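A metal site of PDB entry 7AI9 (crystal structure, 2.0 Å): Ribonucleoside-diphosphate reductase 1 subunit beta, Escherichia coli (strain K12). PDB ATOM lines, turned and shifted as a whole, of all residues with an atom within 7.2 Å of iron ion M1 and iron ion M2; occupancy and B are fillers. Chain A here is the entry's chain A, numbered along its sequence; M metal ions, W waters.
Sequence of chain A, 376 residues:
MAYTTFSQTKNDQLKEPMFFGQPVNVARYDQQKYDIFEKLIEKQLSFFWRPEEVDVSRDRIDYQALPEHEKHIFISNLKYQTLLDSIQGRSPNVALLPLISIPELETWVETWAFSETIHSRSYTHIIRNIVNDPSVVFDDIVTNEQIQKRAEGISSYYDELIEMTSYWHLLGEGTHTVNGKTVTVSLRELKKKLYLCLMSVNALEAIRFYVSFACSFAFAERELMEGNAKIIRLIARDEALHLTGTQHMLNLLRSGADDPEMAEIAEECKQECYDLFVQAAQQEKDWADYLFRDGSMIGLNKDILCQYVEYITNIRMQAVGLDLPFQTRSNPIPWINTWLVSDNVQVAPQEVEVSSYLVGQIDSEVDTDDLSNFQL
O of Asp 85 is in hydrogen-bond range of OG of Ser 120, at 3.1 Å. OE2 of Glu 205 sits close to NE1 of Trp 112. The side-chain carboxylate (OE2) of Glu 205 sits close to the side-chain amide nitrogen (NE2) of Gln 88 (3.0 Å). The side-chain carboxylate (OE2) of Glu 116 sits close to the indole nitrogen (NE1) of Trp 112 (3.2 Å). The backbone carbonyl oxygen (O) of Glu 116 is in hydrogen-bond range of the side-chain hydroxyl (OG) of Ser 120, at 3.4 Å. A ring nitrogen (NE2) of His 242 lies within hydrogen-bond range of the side-chain hydroxyl of Ser 115. OD2 of Asp 238 sits at hydrogen-bond distance from NE2 of His 119 (2.6 Å).
Within 4 Å of iron ion M2: Glu 116, Glu 205, Glu 239 and His 242.
Iron ion M1 is bound by water W1, OD2 of Asp 85, OE1 of Glu 116, ND1 of His 119 and water W3. Slightly farther from iron ion M1 lies the side-chain carboxylate (OD1) of Asp 85 (2.8 Å). Slightly farther from iron ion M1 lies water W2 (2.8 Å).
Water W2 is bound to iron ion M2. Iron ion M2 is bound by OE2 of Glu 205, 2.0 Å away. Water W1 binds iron ion M2 (2.0 Å). OE1 of Glu 239 binds iron ion M2 (2.1 Å). Iron ion M2 is bound by the side-chain carboxylate (OE2) of Glu 116. Iron ion M2 is bound by a ring nitrogen (ND1) of His 242, 2.2 Å away.
Water W2 lies within hydrogen-bond range of OD1 of Asp 85 (2.8 Å) and OE2 of Glu 239 (2.8 Å).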
ATOM      1  N   GLN A  81     -14.369 -26.016 -21.079  1.00  0.00           N
ATOM      2  CA  GLN A  81     -13.863 -24.950 -21.943  1.00  0.00           C
ATOM      3  C   GLN A  81     -14.959 -24.406 -22.831  1.00  0.00           C
ATOM      4  O   GLN A  81     -15.124 -23.190 -22.966  1.00  0.00           O
ATOM      5  CB  GLN A  81     -12.709 -25.473 -22.799  1.00  0.00           C
ATOM      6  CG  GLN A  81     -11.460 -25.808 -22.001  1.00  0.00           C
ATOM      7  CD  GLN A  81     -10.359 -26.500 -22.825  1.00  0.00           C
ATOM      8  OE1 GLN A  81     -10.642 -27.335 -23.674  1.00  0.00           O
ATOM      9  NE2 GLN A  81      -9.097 -26.189 -22.530  1.00  0.00           N
ATOM     10  N   LEU A  84     -17.356 -22.375 -20.807  1.00  0.00           N
ATOM     11  CA  LEU A  84     -16.813 -21.081 -20.417  1.00  0.00           C
ATOM     12  C   LEU A  84     -16.781 -20.108 -21.583  1.00  0.00           C
ATOM     13  O   LEU A  84     -17.053 -18.910 -21.407  1.00  0.00           O
ATOM     14  CB  LEU A  84     -15.410 -21.254 -19.838  1.00  0.00           C
ATOM     15  CG  LEU A  84     -15.312 -21.912 -18.464  1.00  0.00           C
ATOM     16  CD1 LEU A  84     -13.856 -22.081 -17.995  1.00  0.00           C
ATOM     17  CD2 LEU A  84     -16.119 -21.112 -17.462  1.00  0.00           C
ATOM     18  N   ASP A  85     -16.421 -20.564 -22.774  1.00  0.00           N
ATOM     19  CA  ASP A  85     -16.341 -19.611 -23.861  1.00  0.00           C
ATOM     20  C   ASP A  85     -17.673 -19.407 -24.567  1.00  0.00           C
ATOM     21  O   ASP A  85     -17.806 -18.453 -25.348  1.00  0.00           O
ATOM     22  CB  ASP A  85     -15.212 -19.991 -24.836  1.00  0.00           C
ATOM     23  CG  ASP A  85     -13.889 -19.326 -24.448  1.00  0.00           C
ATOM     24  OD1 ASP A  85     -13.902 -18.533 -23.455  1.00  0.00           O
ATOM     25  OD2 ASP A  85     -12.844 -19.580 -25.063  1.00  0.00           O
ATOM     26  N   GLN A  88     -18.274 -16.440 -22.529  1.00  0.00           N
ATOM     27  CA  GLN A  88     -17.342 -15.370 -22.862  1.00  0.00           C
ATOM     28  C   GLN A  88     -17.549 -14.836 -24.266  1.00  0.00           C
ATOM     29  O   GLN A  88     -17.187 -13.685 -24.522  1.00  0.00           O
ATOM     30  CB  GLN A  88     -15.903 -15.859 -22.706  1.00  0.00           C
ATOM     31  CG  GLN A  88     -15.442 -15.926 -21.274  1.00  0.00           C
ATOM     32  CD  GLN A  88     -15.454 -14.569 -20.622  1.00  0.00           C
ATOM     33  OE1 GLN A  88     -16.407 -14.212 -19.909  1.00  0.00           O
ATOM     34  NE2 GLN A  88     -14.420 -13.783 -20.876  1.00  0.00           N
ATOM     35  N   GLY A  89     -18.100 -15.654 -25.154  1.00  0.00           N
ATOM     36  CA  GLY A  89     -18.402 -15.179 -26.501  1.00  0.00           C
ATOM     37  C   GLY A  89     -19.412 -14.043 -26.514  1.00  0.00           C
ATOM     38  O   GLY A  89     -19.268 -13.101 -27.277  1.00  0.00           O
ATOM     39  N   TRP A 112     -12.344  -8.626 -28.178  1.00  0.00           N
ATOM     40  CA  TRP A 112     -12.284  -9.700 -27.211  1.00  0.00           C
ATOM     41  C   TRP A 112     -13.403 -10.715 -27.378  1.00  0.00           C
ATOM     42  O   TRP A 112     -13.146 -11.919 -27.528  1.00  0.00           O
ATOM     43  CB  TRP A 112     -12.334  -9.050 -25.838  1.00  0.00           C
ATOM     44  CG  TRP A 112     -12.411  -9.935 -24.627  1.00  0.00           C
ATOM     45  CD1 TRP A 112     -12.137 -11.265 -24.535  1.00  0.00           C
ATOM     46  CD2 TRP A 112     -12.827  -9.502 -23.337  1.00  0.00           C
ATOM     47  NE1 TRP A 112     -12.325 -11.682 -23.215  1.00  0.00           N
ATOM     48  CE2 TRP A 112     -12.757 -10.615 -22.466  1.00  0.00           C
ATOM     49  CE3 TRP A 112     -13.230  -8.259 -22.821  1.00  0.00           C
ATOM     50  CZ2 TRP A 112     -13.092 -10.522 -21.114  1.00  0.00           C
ATOM     51  CZ3 TRP A 112     -13.564  -8.164 -21.482  1.00  0.00           C
ATOM     52  CH2 TRP A 112     -13.486  -9.302 -20.643  1.00  0.00           C
ATOM     53  N   SER A 115     -13.012 -12.660 -30.594  1.00  0.00           N
ATOM     54  CA  SER A 115     -11.993 -13.699 -30.503  1.00  0.00           C
ATOM     55  C   SER A 115     -12.522 -14.895 -29.715  1.00  0.00           C
ATOM     56  O   SER A 115     -12.182 -16.043 -30.016  1.00  0.00           O
ATOM     57  CB  SER A 115     -10.740 -13.116 -29.895  1.00  0.00           C
ATOM     58  OG  SER A 115     -10.889 -12.936 -28.482  1.00  0.00           O
ATOM     59  N   GLU A 116     -13.449 -14.661 -28.780  1.00  0.00           N
ATOM     60  CA  GLU A 116     -14.029 -15.789 -28.058  1.00  0.00           C
ATOM     61  C   GLU A 116     -14.914 -16.640 -28.953  1.00  0.00           C
ATOM     62  O   GLU A 116     -14.989 -17.856 -28.735  1.00  0.00           O
ATOM     63  CB  GLU A 116     -14.854 -15.335 -26.859  1.00  0.00           C
ATOM     64  CG  GLU A 116     -14.134 -14.497 -25.814  1.00  0.00           C
ATOM     65  CD  GLU A 116     -13.138 -15.293 -24.993  1.00  0.00           C
ATOM     66  OE1 GLU A 116     -12.893 -16.471 -25.305  1.00  0.00           O
ATOM     67  OE2 GLU A 116     -12.640 -14.758 -23.989  1.00  0.00           O
ATOM     68  N   THR A 117     -15.599 -16.033 -29.939  1.00  0.00           N
ATOM     69  CA  THR A 117     -16.401 -16.866 -30.825  1.00  0.00           C
ATOM     70  C   THR A 117     -15.503 -17.756 -31.675  1.00  0.00           C
ATOM     71  O   THR A 117     -15.907 -18.868 -32.025  1.00  0.00           O
ATOM     72  CB  THR A 117     -17.343 -16.048 -31.732  1.00  0.00           C
ATOM     73  OG1 THR A 117     -16.591 -15.307 -32.698  1.00  0.00           O
ATOM     74  CG2 THR A 117     -18.239 -15.112 -30.926  1.00  0.00           C
ATOM     75  N   ILE A 118     -14.304 -17.294 -32.016  1.00  0.00           N
ATOM     76  CA  ILE A 118     -13.364 -18.182 -32.705  1.00  0.00           C
ATOM     77  C   ILE A 118     -12.978 -19.333 -31.781  1.00  0.00           C
ATOM     78  O   ILE A 118     -12.906 -20.496 -32.210  1.00  0.00           O
ATOM     79  CB  ILE A 118     -12.127 -17.389 -33.179  1.00  0.00           C
ATOM     80  CG1 ILE A 118     -12.558 -16.273 -34.154  1.00  0.00           C
ATOM     81  CG2 ILE A 118     -11.106 -18.335 -33.827  1.00  0.00           C
ATOM     82  CD1 ILE A 118     -13.242 -16.798 -35.435  1.00  0.00           C
ATOM     83  N   HIS A 119     -12.773 -19.049 -30.500  1.00  0.00           N
ATOM     84  CA  HIS A 119     -12.526 -20.140 -29.557  1.00  0.00           C
ATOM     85  C   HIS A 119     -13.699 -21.115 -29.552  1.00  0.00           C
ATOM     86  O   HIS A 119     -13.516 -22.327 -29.680  1.00  0.00           O
ATOM     87  CB  HIS A 119     -12.245 -19.597 -28.138  1.00  0.00           C
ATOM     88  CG  HIS A 119     -11.037 -18.729 -28.047  1.00  0.00           C
ATOM     89  ND1 HIS A 119     -10.647 -18.102 -26.881  1.00  0.00           N
ATOM     90  CD2 HIS A 119     -10.127 -18.368 -28.987  1.00  0.00           C
ATOM     91  CE1 HIS A 119      -9.547 -17.397 -27.105  1.00  0.00           C
ATOM     92  NE2 HIS A 119      -9.207 -17.552 -28.366  1.00  0.00           N
ATOM     93  N   SER A 120     -14.929 -20.595 -29.467  1.00  0.00           N
ATOM     94  CA  SER A 120     -16.101 -21.477 -29.457  1.00  0.00           C
ATOM     95  C   SER A 120     -16.184 -22.288 -30.760  1.00  0.00           C
ATOM     96  O   SER A 120     -16.512 -23.488 -30.737  1.00  0.00           O
ATOM     97  CB  SER A 120     -17.377 -20.662 -29.251  1.00  0.00           C
ATOM     98  OG  SER A 120     -17.390 -20.078 -27.956  1.00  0.00           O
ATOM     99  N   TYR A 123     -13.747 -25.214 -30.602  1.00  0.00           N
ATOM    100  CA  TYR A 123     -14.167 -26.375 -29.816  1.00  0.00           C
ATOM    101  C   TYR A 123     -15.131 -27.245 -30.604  1.00  0.00           C
ATOM    102  O   TYR A 123     -15.116 -28.474 -30.460  1.00  0.00           O
ATOM    103  CB  TYR A 123     -14.813 -25.936 -28.491  1.00  0.00           C
ATOM    104  CG  TYR A 123     -13.914 -25.112 -27.606  1.00  0.00           C
ATOM    105  CD1 TYR A 123     -12.633 -25.540 -27.297  1.00  0.00           C
ATOM    106  CD2 TYR A 123     -14.341 -23.882 -27.108  1.00  0.00           C
ATOM    107  CE1 TYR A 123     -11.793 -24.771 -26.502  1.00  0.00           C
ATOM    108  CE2 TYR A 123     -13.514 -23.114 -26.328  1.00  0.00           C
ATOM    109  CZ  TYR A 123     -12.235 -23.562 -26.029  1.00  0.00           C
ATOM    110  OH  TYR A 123     -11.396 -22.825 -25.231  1.00  0.00           O
ATOM    111  N   LEU A 204     -12.063 -16.186 -14.217  1.00  0.00           N
ATOM    112  CA  LEU A 204     -12.461 -17.106 -15.264  1.00  0.00           C
ATOM    113  C   LEU A 204     -11.336 -17.320 -16.261  1.00  0.00           C
ATOM    114  O   LEU A 204     -10.884 -18.451 -16.487  1.00  0.00           O
ATOM    115  CB  LEU A 204     -13.700 -16.568 -16.006  1.00  0.00           C
ATOM    116  CG  LEU A 204     -14.500 -17.386 -17.026  1.00  0.00           C
ATOM    117  CD1 LEU A 204     -15.856 -16.704 -17.265  1.00  0.00           C
ATOM    118  CD2 LEU A 204     -13.797 -17.501 -18.369  1.00  0.00           C
ATOM    119  N   GLU A 205     -10.868 -16.229 -16.874  1.00  0.00           N
ATOM    120  CA  GLU A 205      -9.829 -16.336 -17.899  1.00  0.00           C
ATOM    121  C   GLU A 205      -8.442 -16.606 -17.312  1.00  0.00           C
ATOM    122  O   GLU A 205      -7.661 -17.333 -17.920  1.00  0.00           O
ATOM    123  CB  GLU A 205      -9.820 -15.066 -18.729  1.00  0.00           C
ATOM    124  CG  GLU A 205     -11.178 -14.926 -19.474  1.00  0.00           C
ATOM    125  CD  GLU A 205     -11.183 -13.813 -20.490  1.00  0.00           C
ATOM    126  OE1 GLU A 205     -10.869 -12.661 -20.119  1.00  0.00           O
ATOM    127  OE2 GLU A 205     -11.533 -14.080 -21.664  1.00  0.00           O
ATOM    128  N   PHE A 209      -9.522 -21.097 -16.928  1.00  0.00           N
ATOM    129  CA  PHE A 209      -9.055 -21.601 -18.217  1.00  0.00           C
ATOM    130  C   PHE A 209      -7.639 -22.148 -18.142  1.00  0.00           C
ATOM    131  O   PHE A 209      -7.309 -23.086 -18.867  1.00  0.00           O
ATOM    132  CB  PHE A 209      -9.128 -20.518 -19.291  1.00  0.00           C
ATOM    133  CG  PHE A 209     -10.319 -20.672 -20.204  1.00  0.00           C
ATOM    134  CD1 PHE A 209     -10.365 -21.690 -21.145  1.00  0.00           C
ATOM    135  CD2 PHE A 209     -11.377 -19.806 -20.105  1.00  0.00           C
ATOM    136  CE1 PHE A 209     -11.448 -21.864 -21.939  1.00  0.00           C
ATOM    137  CE2 PHE A 209     -12.491 -19.952 -20.940  1.00  0.00           C
ATOM    138  CZ  PHE A 209     -12.530 -20.983 -21.847  1.00  0.00           C
ATOM    139  N   PHE A 213      -6.148 -25.564 -19.544  1.00  0.00           N
ATOM    140  CA  PHE A 213      -4.993 -25.672 -20.418  1.00  0.00           C
ATOM    141  C   PHE A 213      -4.028 -26.748 -19.928  1.00  0.00           C
ATOM    142  O   PHE A 213      -3.487 -27.515 -20.738  1.00  0.00           O
ATOM    143  CB  PHE A 213      -4.283 -24.316 -20.522  1.00  0.00           C
ATOM    144  CG  PHE A 213      -5.122 -23.200 -21.118  1.00  0.00           C
ATOM    145  CD1 PHE A 213      -6.233 -23.471 -21.933  1.00  0.00           C
ATOM    146  CD2 PHE A 213      -4.779 -21.868 -20.916  1.00  0.00           C
ATOM    147  CE1 PHE A 213      -6.993 -22.433 -22.499  1.00  0.00           C
ATOM    148  CE2 PHE A 213      -5.529 -20.819 -21.465  1.00  0.00           C
ATOM    149  CZ  PHE A 213      -6.643 -21.112 -22.276  1.00  0.00           C
ATOM    150  N   ILE A 235      -5.516 -20.632 -28.365  1.00  0.00           N
ATOM    151  CA  ILE A 235      -6.501 -20.091 -27.431  1.00  0.00           C
ATOM    152  C   ILE A 235      -5.807 -19.473 -26.230  1.00  0.00           C
ATOM    153  O   ILE A 235      -6.145 -18.360 -25.797  1.00  0.00           O
ATOM    154  CB  ILE A 235      -7.473 -21.210 -27.022  1.00  0.00           C
ATOM    155  CG1 ILE A 235      -8.397 -21.543 -28.196  1.00  0.00           C
ATOM    156  CG2 ILE A 235      -8.276 -20.818 -25.772  1.00  0.00           C
ATOM    157  CD1 ILE A 235      -9.356 -22.710 -27.886  1.00  0.00           C
ATOM    158  N   ALA A 236      -4.797 -20.173 -25.689  1.00  0.00           N
ATOM    159  CA  ALA A 236      -4.074 -19.679 -24.516  1.00  0.00           C
ATOM    160  C   ALA A 236      -3.349 -18.368 -24.825  1.00  0.00           C
ATOM    161  O   ALA A 236      -3.298 -17.462 -23.984  1.00  0.00           O
ATOM    162  CB  ALA A 236      -3.095 -20.750 -24.040  1.00  0.00           C
ATOM    163  N   ASP A 238      -4.383 -16.120 -26.906  1.00  0.00           N
ATOM    164  CA  ASP A 238      -5.441 -15.108 -26.831  1.00  0.00           C
ATOM    165  C   ASP A 238      -5.817 -14.838 -25.380  1.00  0.00           C
ATOM    166  O   ASP A 238      -5.982 -13.675 -24.965  1.00  0.00           O
ATOM    167  CB  ASP A 238      -6.707 -15.563 -27.595  1.00  0.00           C
ATOM    168  CG  ASP A 238      -6.504 -15.680 -29.096  1.00  0.00           C
ATOM    169  OD1 ASP A 238      -5.586 -15.033 -29.634  1.00  0.00           O
ATOM    170  OD2 ASP A 238      -7.332 -16.400 -29.749  1.00  0.00           O
ATOM    171  N   GLU A 239      -5.954 -15.896 -24.589  1.00  0.00           N
ATOM    172  CA  GLU A 239      -6.391 -15.746 -23.208  1.00  0.00           C
ATOM    173  C   GLU A 239      -5.459 -14.833 -22.409  1.00  0.00           C
ATOM    174  O   GLU A 239      -5.910 -14.128 -21.501  1.00  0.00           O
ATOM    175  CB  GLU A 239      -6.471 -17.116 -22.545  1.00  0.00           C
ATOM    176  CG  GLU A 239      -7.259 -17.116 -21.266  1.00  0.00           C
ATOM    177  CD  GLU A 239      -8.724 -16.976 -21.582  1.00  0.00           C
ATOM    178  OE1 GLU A 239      -9.169 -15.829 -21.753  1.00  0.00           O
ATOM    179  OE2 GLU A 239      -9.435 -17.989 -21.684  1.00  0.00           O
ATOM    180  N   ALA A 240      -4.170 -14.826 -22.752  1.00  0.00           N
ATOM    181  CA  ALA A 240      -3.215 -13.966 -22.073  1.00  0.00           C
ATOM    182  C   ALA A 240      -3.531 -12.492 -22.336  1.00  0.00           C
ATOM    183  O   ALA A 240      -3.334 -11.651 -21.442  1.00  0.00           O
ATOM    184  CB  ALA A 240      -1.793 -14.300 -22.513  1.00  0.00           C
ATOM    185  N   LEU A 241      -4.002 -12.174 -23.544  1.00  0.00           N
ATOM    186  CA  LEU A 241      -4.488 -10.836 -23.851  1.00  0.00           C
ATOM    187  C   LEU A 241      -5.764 -10.528 -23.074  1.00  0.00           C
ATOM    188  O   LEU A 241      -5.913  -9.439 -22.510  1.00  0.00           O
ATOM    189  CB  LEU A 241      -4.779 -10.682 -25.353  1.00  0.00           C
ATOM    190  CG  LEU A 241      -3.657 -10.904 -26.372  1.00  0.00           C
ATOM    191  CD1 LEU A 241      -4.192 -10.598 -27.787  1.00  0.00           C
ATOM    192  CD2 LEU A 241      -2.395 -10.121 -26.060  1.00  0.00           C
ATOM    193  N   HIS A 242      -6.698 -11.471 -23.062  1.00  0.00           N
ATOM    194  CA  HIS A 242      -7.963 -11.244 -22.366  1.00  0.00           C
ATOM    195  C   HIS A 242      -7.728 -10.911 -20.906  1.00  0.00           C
ATOM    196  O   HIS A 242      -8.252  -9.923 -20.374  1.00  0.00           O
ATOM    197  CB  HIS A 242      -8.836 -12.477 -22.487  1.00  0.00           C
ATOM    198  CG  HIS A 242      -9.166 -12.825 -23.906  1.00  0.00           C
ATOM    199  ND1 HIS A 242      -9.752 -14.011 -24.243  1.00  0.00           N
ATOM    200  CD2 HIS A 242      -8.897 -12.182 -25.062  1.00  0.00           C
ATOM    201  CE1 HIS A 242      -9.909 -14.053 -25.567  1.00  0.00           C
ATOM    202  NE2 HIS A 242      -9.354 -12.974 -26.082  1.00  0.00           N
ATOM    203  N   LEU A 243      -6.960 -11.734 -20.220  1.00  0.00           N
ATOM    204  CA  LEU A 243      -6.817 -11.500 -18.793  1.00  0.00           C
ATOM    205  C   LEU A 243      -6.016 -10.238 -18.524  1.00  0.00           C
ATOM    206  O   LEU A 243      -6.174  -9.607 -17.475  1.00  0.00           O
ATOM    207  CB  LEU A 243      -6.217 -12.748 -18.145  1.00  0.00           C
ATOM    208  CG  LEU A 243      -4.766 -13.081 -18.440  1.00  0.00           C
ATOM    209  CD1 LEU A 243      -3.890 -12.350 -17.412  1.00  0.00           C
ATOM    210  CD2 LEU A 243      -4.557 -14.562 -18.322  1.00  0.00           C
HETATM  211 FE    FE M   1     -11.602 -18.099 -24.942  1.00  0.00          FE
HETATM  212 FE    FE M   2     -10.835 -15.402 -23.005  1.00  0.00          FE
HETATM  213  O   HOH W   1     -10.334 -16.875 -24.315  1.00  0.00           O
HETATM  214  O   HOH W   2     -11.925 -16.896 -22.431  1.00  0.00           O
HETATM  215  O   HOH W   3     -10.402 -19.644 -23.845  1.00  0.00           O
